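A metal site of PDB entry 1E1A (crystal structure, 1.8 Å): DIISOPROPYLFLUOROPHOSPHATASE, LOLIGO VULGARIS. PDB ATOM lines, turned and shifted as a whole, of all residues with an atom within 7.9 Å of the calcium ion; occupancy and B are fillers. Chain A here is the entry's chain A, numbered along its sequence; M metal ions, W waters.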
ATOM      1  N   GLY A  19      36.362  -3.423  16.911  1.00  0.00           N
ATOM      2  CA  GLY A  19      35.492  -4.360  17.600  1.00  0.00           C
ATOM      3  C   GLY A  19      34.120  -4.479  16.956  1.00  0.00           C
ATOM      4  O   GLY A  19      33.159  -4.844  17.637  1.00  0.00           O
ATOM      5  N   ALA A  20      34.049  -4.202  15.651  1.00  0.00           N
ATOM      6  CA  ALA A  20      32.820  -4.261  14.852  1.00  0.00           C
ATOM      7  C   ALA A  20      31.829  -5.274  15.413  1.00  0.00           C
ATOM      8  O   ALA A  20      32.106  -6.481  15.477  1.00  0.00           O
ATOM      9  CB  ALA A  20      33.158  -4.602  13.403  1.00  0.00           C
ATOM     10  N   GLU A  21      30.679  -4.771  15.837  1.00  0.00           N
ATOM     11  CA  GLU A  21      29.663  -5.615  16.468  1.00  0.00           C
ATOM     12  C   GLU A  21      28.235  -5.169  16.186  1.00  0.00           C
ATOM     13  O   GLU A  21      27.988  -4.217  15.451  1.00  0.00           O
ATOM     14  CB  GLU A  21      29.893  -5.580  17.988  1.00  0.00           C
ATOM     15  CG  GLU A  21      30.622  -6.783  18.568  1.00  0.00           C
ATOM     16  CD  GLU A  21      29.680  -7.914  18.945  1.00  0.00           C
ATOM     17  OE1 GLU A  21      28.579  -8.021  18.372  1.00  0.00           O
ATOM     18  OE2 GLU A  21      30.051  -8.712  19.844  1.00  0.00           O
ATOM     19  N   GLY A  22      27.307  -5.901  16.814  1.00  0.00           N
ATOM     20  CA  GLY A  22      25.879  -5.625  16.729  1.00  0.00           C
ATOM     21  C   GLY A  22      25.251  -5.211  15.416  1.00  0.00           C
ATOM     22  O   GLY A  22      24.554  -4.203  15.385  1.00  0.00           O
ATOM     23  N   ALA A  74      27.919  -2.885  22.308  1.00  0.00           N
ATOM     24  CA  ALA A  74      28.304  -4.145  21.679  1.00  0.00           C
ATOM     25  C   ALA A  74      27.244  -4.971  20.951  1.00  0.00           C
ATOM     26  O   ALA A  74      27.589  -5.847  20.171  1.00  0.00           O
ATOM     27  CB  ALA A  74      29.004  -5.006  22.713  1.00  0.00           C
ATOM     28  N   GLY A  75      25.964  -4.736  21.222  1.00  0.00           N
ATOM     29  CA  GLY A  75      24.929  -5.525  20.567  1.00  0.00           C
ATOM     30  C   GLY A  75      23.670  -4.703  20.362  1.00  0.00           C
ATOM     31  O   GLY A  75      23.414  -3.778  21.119  1.00  0.00           O
ATOM     32  N   MET A  90      28.603  -2.523  27.305  1.00  0.00           N
ATOM     33  CA  MET A  90      29.478  -3.140  28.301  1.00  0.00           C
ATOM     34  C   MET A  90      29.809  -2.280  29.527  1.00  0.00           C
ATOM     35  O   MET A  90      30.207  -2.797  30.571  1.00  0.00           O
ATOM     36  CB  MET A  90      30.751  -3.590  27.592  1.00  0.00           C
ATOM     37  CG  MET A  90      31.280  -4.899  28.063  1.00  0.00           C
ATOM     38  SD  MET A  90      30.375  -6.389  27.586  1.00  0.00           S
ATOM     39  CE  MET A  90      31.729  -7.471  27.910  1.00  0.00           C
ATOM     40  N   CYS A 119      26.287  -4.968  29.553  1.00  0.00           N
ATOM     41  CA  CYS A 119      25.732  -5.970  28.647  1.00  0.00           C
ATOM     42  C   CYS A 119      26.468  -6.092  27.322  1.00  0.00           C
ATOM     43  O   CYS A 119      27.176  -5.170  26.900  1.00  0.00           O
ATOM     44  CB  CYS A 119      24.258  -5.656  28.404  1.00  0.00           C
ATOM     45  SG  CYS A 119      23.289  -5.591  29.932  1.00  0.00           S
ATOM     46  N   ASN A 120      26.273  -7.213  26.630  1.00  0.00           N
ATOM     47  CA  ASN A 120      26.956  -7.430  25.358  1.00  0.00           C
ATOM     48  C   ASN A 120      26.045  -7.648  24.147  1.00  0.00           C
ATOM     49  O   ASN A 120      26.307  -7.134  23.059  1.00  0.00           O
ATOM     50  CB  ASN A 120      27.957  -8.578  25.490  1.00  0.00           C
ATOM     51  CG  ASN A 120      28.902  -8.641  24.318  1.00  0.00           C
ATOM     52  OD1 ASN A 120      28.587  -9.257  23.306  1.00  0.00           O
ATOM     53  ND2 ASN A 120      30.050  -7.983  24.440  1.00  0.00           N
ATOM     54  N   ASP A 121      24.997  -8.443  24.324  1.00  0.00           N
ATOM     55  CA  ASP A 121      24.069  -8.698  23.235  1.00  0.00           C
ATOM     56  C   ASP A 121      22.657  -8.868  23.797  1.00  0.00           C
ATOM     57  O   ASP A 121      22.486  -9.027  25.011  1.00  0.00           O
ATOM     58  CB  ASP A 121      24.486  -9.919  22.408  1.00  0.00           C
ATOM     59  CG  ASP A 121      24.094  -9.800  20.926  1.00  0.00           C
ATOM     60  OD1 ASP A 121      23.305  -8.897  20.562  1.00  0.00           O
ATOM     61  OD2 ASP A 121      24.582 -10.610  20.115  1.00  0.00           O
ATOM     62  N   CYS A 122      21.666  -8.810  22.922  1.00  0.00           N
ATOM     63  CA  CYS A 122      20.282  -8.954  23.334  1.00  0.00           C
ATOM     64  C   CYS A 122      19.440  -9.518  22.211  1.00  0.00           C
ATOM     65  O   CYS A 122      19.852  -9.529  21.041  1.00  0.00           O
ATOM     66  CB  CYS A 122      19.727  -7.602  23.817  1.00  0.00           C
ATOM     67  SG  CYS A 122      19.834  -6.236  22.628  1.00  0.00           S
ATOM     68  N   THR A 133      22.389 -10.467  27.547  1.00  0.00           N
ATOM     69  CA  THR A 133      23.547 -11.097  28.172  1.00  0.00           C
ATOM     70  C   THR A 133      24.369  -9.986  28.822  1.00  0.00           C
ATOM     71  O   THR A 133      24.553  -8.917  28.229  1.00  0.00           O
ATOM     72  CB  THR A 133      24.430 -11.871  27.181  1.00  0.00           C
ATOM     73  OG1 THR A 133      24.807 -11.021  26.087  1.00  0.00           O
ATOM     74  CG2 THR A 133      23.712 -13.111  26.657  1.00  0.00           C
ATOM     75  N   PRO A 135      27.962  -9.964  30.370  1.00  0.00           N
ATOM     76  CA  PRO A 135      29.262 -10.539  30.716  1.00  0.00           C
ATOM     77  C   PRO A 135      30.205  -9.623  31.490  1.00  0.00           C
ATOM     78  O   PRO A 135      31.230 -10.064  31.999  1.00  0.00           O
ATOM     79  CB  PRO A 135      29.838 -10.913  29.356  1.00  0.00           C
ATOM     80  CG  PRO A 135      29.310  -9.816  28.481  1.00  0.00           C
ATOM     81  CD  PRO A 135      27.882  -9.675  28.931  1.00  0.00           C
ATOM     82  N   PHE A 173      31.347 -15.292  30.759  1.00  0.00           N
ATOM     83  CA  PHE A 173      31.163 -14.476  29.578  1.00  0.00           C
ATOM     84  C   PHE A 173      29.978 -14.844  28.683  1.00  0.00           C
ATOM     85  O   PHE A 173      30.154 -15.376  27.574  1.00  0.00           O
ATOM     86  CB  PHE A 173      32.445 -14.359  28.751  1.00  0.00           C
ATOM     87  CG  PHE A 173      32.556 -13.044  28.007  1.00  0.00           C
ATOM     88  CD1 PHE A 173      31.927 -12.866  26.779  1.00  0.00           C
ATOM     89  CD2 PHE A 173      33.255 -11.984  28.564  1.00  0.00           C
ATOM     90  CE1 PHE A 173      31.988 -11.637  26.110  1.00  0.00           C
ATOM     91  CE2 PHE A 173      33.321 -10.751  27.906  1.00  0.00           C
ATOM     92  CZ  PHE A 173      32.683 -10.582  26.679  1.00  0.00           C
ATOM     93  N   PRO A 174      28.743 -14.624  29.170  1.00  0.00           N
ATOM     94  CA  PRO A 174      27.549 -14.909  28.375  1.00  0.00           C
ATOM     95  C   PRO A 174      27.669 -13.925  27.200  1.00  0.00           C
ATOM     96  O   PRO A 174      28.023 -12.757  27.404  1.00  0.00           O
ATOM     97  CB  PRO A 174      26.402 -14.563  29.332  1.00  0.00           C
ATOM     98  CG  PRO A 174      27.012 -13.526  30.255  1.00  0.00           C
ATOM     99  CD  PRO A 174      28.387 -14.092  30.499  1.00  0.00           C
ATOM    100  N   ASN A 175      27.433 -14.381  25.978  1.00  0.00           N
ATOM    101  CA  ASN A 175      27.629 -13.521  24.826  1.00  0.00           C
ATOM    102  C   ASN A 175      26.423 -13.421  23.889  1.00  0.00           C
ATOM    103  O   ASN A 175      25.512 -12.636  24.135  1.00  0.00           O
ATOM    104  CB  ASN A 175      28.882 -14.003  24.088  1.00  0.00           C
ATOM    105  CG  ASN A 175      29.543 -12.912  23.294  1.00  0.00           C
ATOM    106  OD1 ASN A 175      28.890 -12.012  22.775  1.00  0.00           O
ATOM    107  ND2 ASN A 175      30.866 -12.982  23.176  1.00  0.00           N
ATOM    108  N   GLY A 176      26.428 -14.191  22.805  1.00  0.00           N
ATOM    109  CA  GLY A 176      25.313 -14.181  21.870  1.00  0.00           C
ATOM    110  C   GLY A 176      24.073 -14.738  22.541  1.00  0.00           C
ATOM    111  O   GLY A 176      24.163 -15.555  23.460  1.00  0.00           O
ATOM    112  N   ILE A 177      22.907 -14.314  22.078  1.00  0.00           N
ATOM    113  CA  ILE A 177      21.649 -14.768  22.654  1.00  0.00           C
ATOM    114  C   ILE A 177      20.576 -14.798  21.568  1.00  0.00           C
ATOM    115  O   ILE A 177      20.587 -13.972  20.659  1.00  0.00           O
ATOM    116  CB  ILE A 177      21.265 -13.852  23.859  1.00  0.00           C
ATOM    117  CG1 ILE A 177      20.049 -14.399  24.614  1.00  0.00           C
ATOM    118  CG2 ILE A 177      21.052 -12.419  23.394  1.00  0.00           C
ATOM    119  CD1 ILE A 177      19.900 -13.839  26.017  1.00  0.00           C
ATOM    120  N   THR A 195      31.014 -17.914  25.706  1.00  0.00           N
ATOM    121  CA  THR A 195      32.218 -17.900  24.882  1.00  0.00           C
ATOM    122  C   THR A 195      33.400 -18.820  25.179  1.00  0.00           C
ATOM    123  O   THR A 195      33.588 -19.815  24.484  1.00  0.00           O
ATOM    124  CB  THR A 195      32.707 -16.450  24.619  1.00  0.00           C
ATOM    125  OG1 THR A 195      31.620 -15.665  24.127  1.00  0.00           O
ATOM    126  CG2 THR A 195      33.815 -16.430  23.575  1.00  0.00           C
ATOM    127  N   ALA A 228      31.843 -19.175  20.867  1.00  0.00           N
ATOM    128  CA  ALA A 228      30.610 -18.587  20.346  1.00  0.00           C
ATOM    129  C   ALA A 228      30.431 -17.125  20.726  1.00  0.00           C
ATOM    130  O   ALA A 228      30.531 -16.747  21.896  1.00  0.00           O
ATOM    131  CB  ALA A 228      29.404 -19.388  20.810  1.00  0.00           C
ATOM    132  N   ASP A 229      30.190 -16.303  19.716  1.00  0.00           N
ATOM    133  CA  ASP A 229      29.976 -14.885  19.953  1.00  0.00           C
ATOM    134  C   ASP A 229      28.510 -14.583  19.626  1.00  0.00           C
ATOM    135  O   ASP A 229      27.631 -14.903  20.432  1.00  0.00           O
ATOM    136  CB  ASP A 229      30.946 -14.045  19.112  1.00  0.00           C
ATOM    137  CG  ASP A 229      30.971 -12.585  19.545  1.00  0.00           C
ATOM    138  OD1 ASP A 229      29.951 -12.089  20.053  1.00  0.00           O
ATOM    139  OD2 ASP A 229      32.014 -11.926  19.377  1.00  0.00           O
ATOM    140  N   GLY A 230      28.241 -14.031  18.443  1.00  0.00           N
ATOM    141  CA  GLY A 230      26.876 -13.694  18.058  1.00  0.00           C
ATOM    142  C   GLY A 230      26.126 -14.819  17.383  1.00  0.00           C
ATOM    143  O   GLY A 230      26.731 -15.724  16.813  1.00  0.00           O
ATOM    144  N   MET A 231      24.790 -14.740  17.413  1.00  0.00           N
ATOM    145  CA  MET A 231      23.945 -15.766  16.811  1.00  0.00           C
ATOM    146  C   MET A 231      22.606 -15.220  16.304  1.00  0.00           C
ATOM    147  O   MET A 231      22.146 -14.156  16.724  1.00  0.00           O
ATOM    148  CB  MET A 231      23.668 -16.880  17.823  1.00  0.00           C
ATOM    149  CG  MET A 231      22.883 -16.423  19.061  1.00  0.00           C
ATOM    150  SD  MET A 231      22.523 -17.716  20.264  1.00  0.00           S
ATOM    151  CE  MET A 231      24.171 -18.287  20.643  1.00  0.00           C
ATOM    152  N   TRP A 244      34.112 -17.116  17.162  1.00  0.00           N
ATOM    153  CA  TRP A 244      35.270 -16.209  17.231  1.00  0.00           C
ATOM    154  C   TRP A 244      36.569 -16.978  17.496  1.00  0.00           C
ATOM    155  O   TRP A 244      36.687 -17.667  18.498  1.00  0.00           O
ATOM    156  CB  TRP A 244      35.036 -15.188  18.344  1.00  0.00           C
ATOM    157  CG  TRP A 244      35.890 -13.952  18.303  1.00  0.00           C
ATOM    158  CD1 TRP A 244      35.516 -12.707  17.857  1.00  0.00           C
ATOM    159  CD2 TRP A 244      37.213 -13.779  18.860  1.00  0.00           C
ATOM    160  NE1 TRP A 244      36.506 -11.784  18.108  1.00  0.00           N
ATOM    161  CE2 TRP A 244      37.553 -12.423  18.719  1.00  0.00           C
ATOM    162  CE3 TRP A 244      38.132 -14.650  19.464  1.00  0.00           C
ATOM    163  CZ2 TRP A 244      38.781 -11.909  19.170  1.00  0.00           C
ATOM    164  CZ3 TRP A 244      39.344 -14.141  19.900  1.00  0.00           C
ATOM    165  CH2 TRP A 244      39.653 -12.783  19.758  1.00  0.00           C
ATOM    166  N   SER A 271      32.529 -12.232  14.541  1.00  0.00           N
ATOM    167  CA  SER A 271      31.969 -11.778  15.805  1.00  0.00           C
ATOM    168  C   SER A 271      30.449 -11.852  15.911  1.00  0.00           C
ATOM    169  O   SER A 271      29.921 -12.521  16.784  1.00  0.00           O
ATOM    170  CB  SER A 271      32.443 -10.346  16.070  1.00  0.00           C
ATOM    171  OG  SER A 271      31.852  -9.835  17.254  1.00  0.00           O
ATOM    172  N   ASN A 272      29.756 -11.161  15.019  1.00  0.00           N
ATOM    173  CA  ASN A 272      28.312 -11.143  15.069  1.00  0.00           C
ATOM    174  C   ASN A 272      27.745 -11.145  13.665  1.00  0.00           C
ATOM    175  O   ASN A 272      28.461 -10.869  12.692  1.00  0.00           O
ATOM    176  CB  ASN A 272      27.813  -9.923  15.855  1.00  0.00           C
ATOM    177  CG  ASN A 272      26.625 -10.229  16.760  1.00  0.00           C
ATOM    178  OD1 ASN A 272      26.486  -9.665  17.846  1.00  0.00           O
ATOM    179  ND2 ASN A 272      25.733 -11.111  16.299  1.00  0.00           N
ATOM    180  N   THR A 285      30.218  -9.262  11.101  1.00  0.00           N
ATOM    181  CA  THR A 285      31.273  -8.381  11.611  1.00  0.00           C
ATOM    182  C   THR A 285      32.390  -9.328  12.078  1.00  0.00           C
ATOM    183  O   THR A 285      32.119 -10.448  12.501  1.00  0.00           O
ATOM    184  CB  THR A 285      30.787  -7.496  12.780  1.00  0.00           C
ATOM    185  OG1 THR A 285      30.401  -8.325  13.897  1.00  0.00           O
ATOM    186  CG2 THR A 285      29.617  -6.633  12.363  1.00  0.00           C
ATOM    187  N   HIS A 287      36.633  -9.415  13.885  1.00  0.00           N
ATOM    188  CA  HIS A 287      37.683  -8.681  14.568  1.00  0.00           C
ATOM    189  C   HIS A 287      39.133  -8.894  14.133  1.00  0.00           C
ATOM    190  O   HIS A 287      40.047  -8.424  14.808  1.00  0.00           O
ATOM    191  CB  HIS A 287      37.539  -8.862  16.086  1.00  0.00           C
ATOM    192  CG  HIS A 287      36.187  -8.492  16.606  1.00  0.00           C
ATOM    193  ND1 HIS A 287      35.715  -8.900  17.825  1.00  0.00           N
ATOM    194  CD2 HIS A 287      35.195  -7.735  16.058  1.00  0.00           C
ATOM    195  CE1 HIS A 287      34.496  -8.420  18.017  1.00  0.00           C
ATOM    196  NE2 HIS A 287      34.166  -7.711  16.952  1.00  0.00           N
HETATM  197 CA    CA M   1      28.973 -10.280  21.198  1.00  0.00          CA
HETATM  198  O   HOH W   1      27.039 -11.557  20.590  1.00  0.00           O
HETATM  199  O   HOH W   2      31.489 -10.429  21.797  1.00  0.00           O
HETATM  200  O   HOH W   3      27.108  -8.501  20.765  1.00  0.00           O
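The calcium ion is bound by OE2 of Glu 21, OD1 of Asn 175, OD1 of Asp 229, OD1 of Asn 120, water W1, water W2 and water W3.
The calcium ion has seven donor atoms within binding distance.
Within 4 Å of the calcium ion: Glu 21, Asn 120, Asn 175 and Asp 229.
Along chain A the residues within 4 Å of the calcium ion span positions 21 to 229.
The side-chain carboxylate (OE2) of Glu 21 sits close to the side-chain hydroxyl (OG) of Ser 271 (3.3 Å).
The side-chain hydroxyl (OG) of Ser 271 lies within hydrogen-bond range of the side-chain carboxylate (OD2) of Asp 229 (3.0 Å).
The backbone NH of Gly 176 sits at hydrogen-bond distance from the backbone carbonyl oxygen of Asp 229 (2.8 Å).
O of Asn 120 sits at hydrogen-bond distance from N of Gly 75, 3.0 Å away.
N of Asn 120 lies within hydrogen-bond range of O of Thr 133 (2.9 Å).
OG1 of Thr 195 is in hydrogen-bond range of ND2 of Asn 175.
O of Asn 175 is in hydrogen-bond range of OG1 of Thr 133.
The side-chain amide oxygen (OD1) of Asn 272 sits close to the side-chain carboxylate (OE1) of Glu 21 (2.7 Å).
Water W2 lies within hydrogen-bond range of OD2 of Asp 229 and ND2 of Asn 175.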
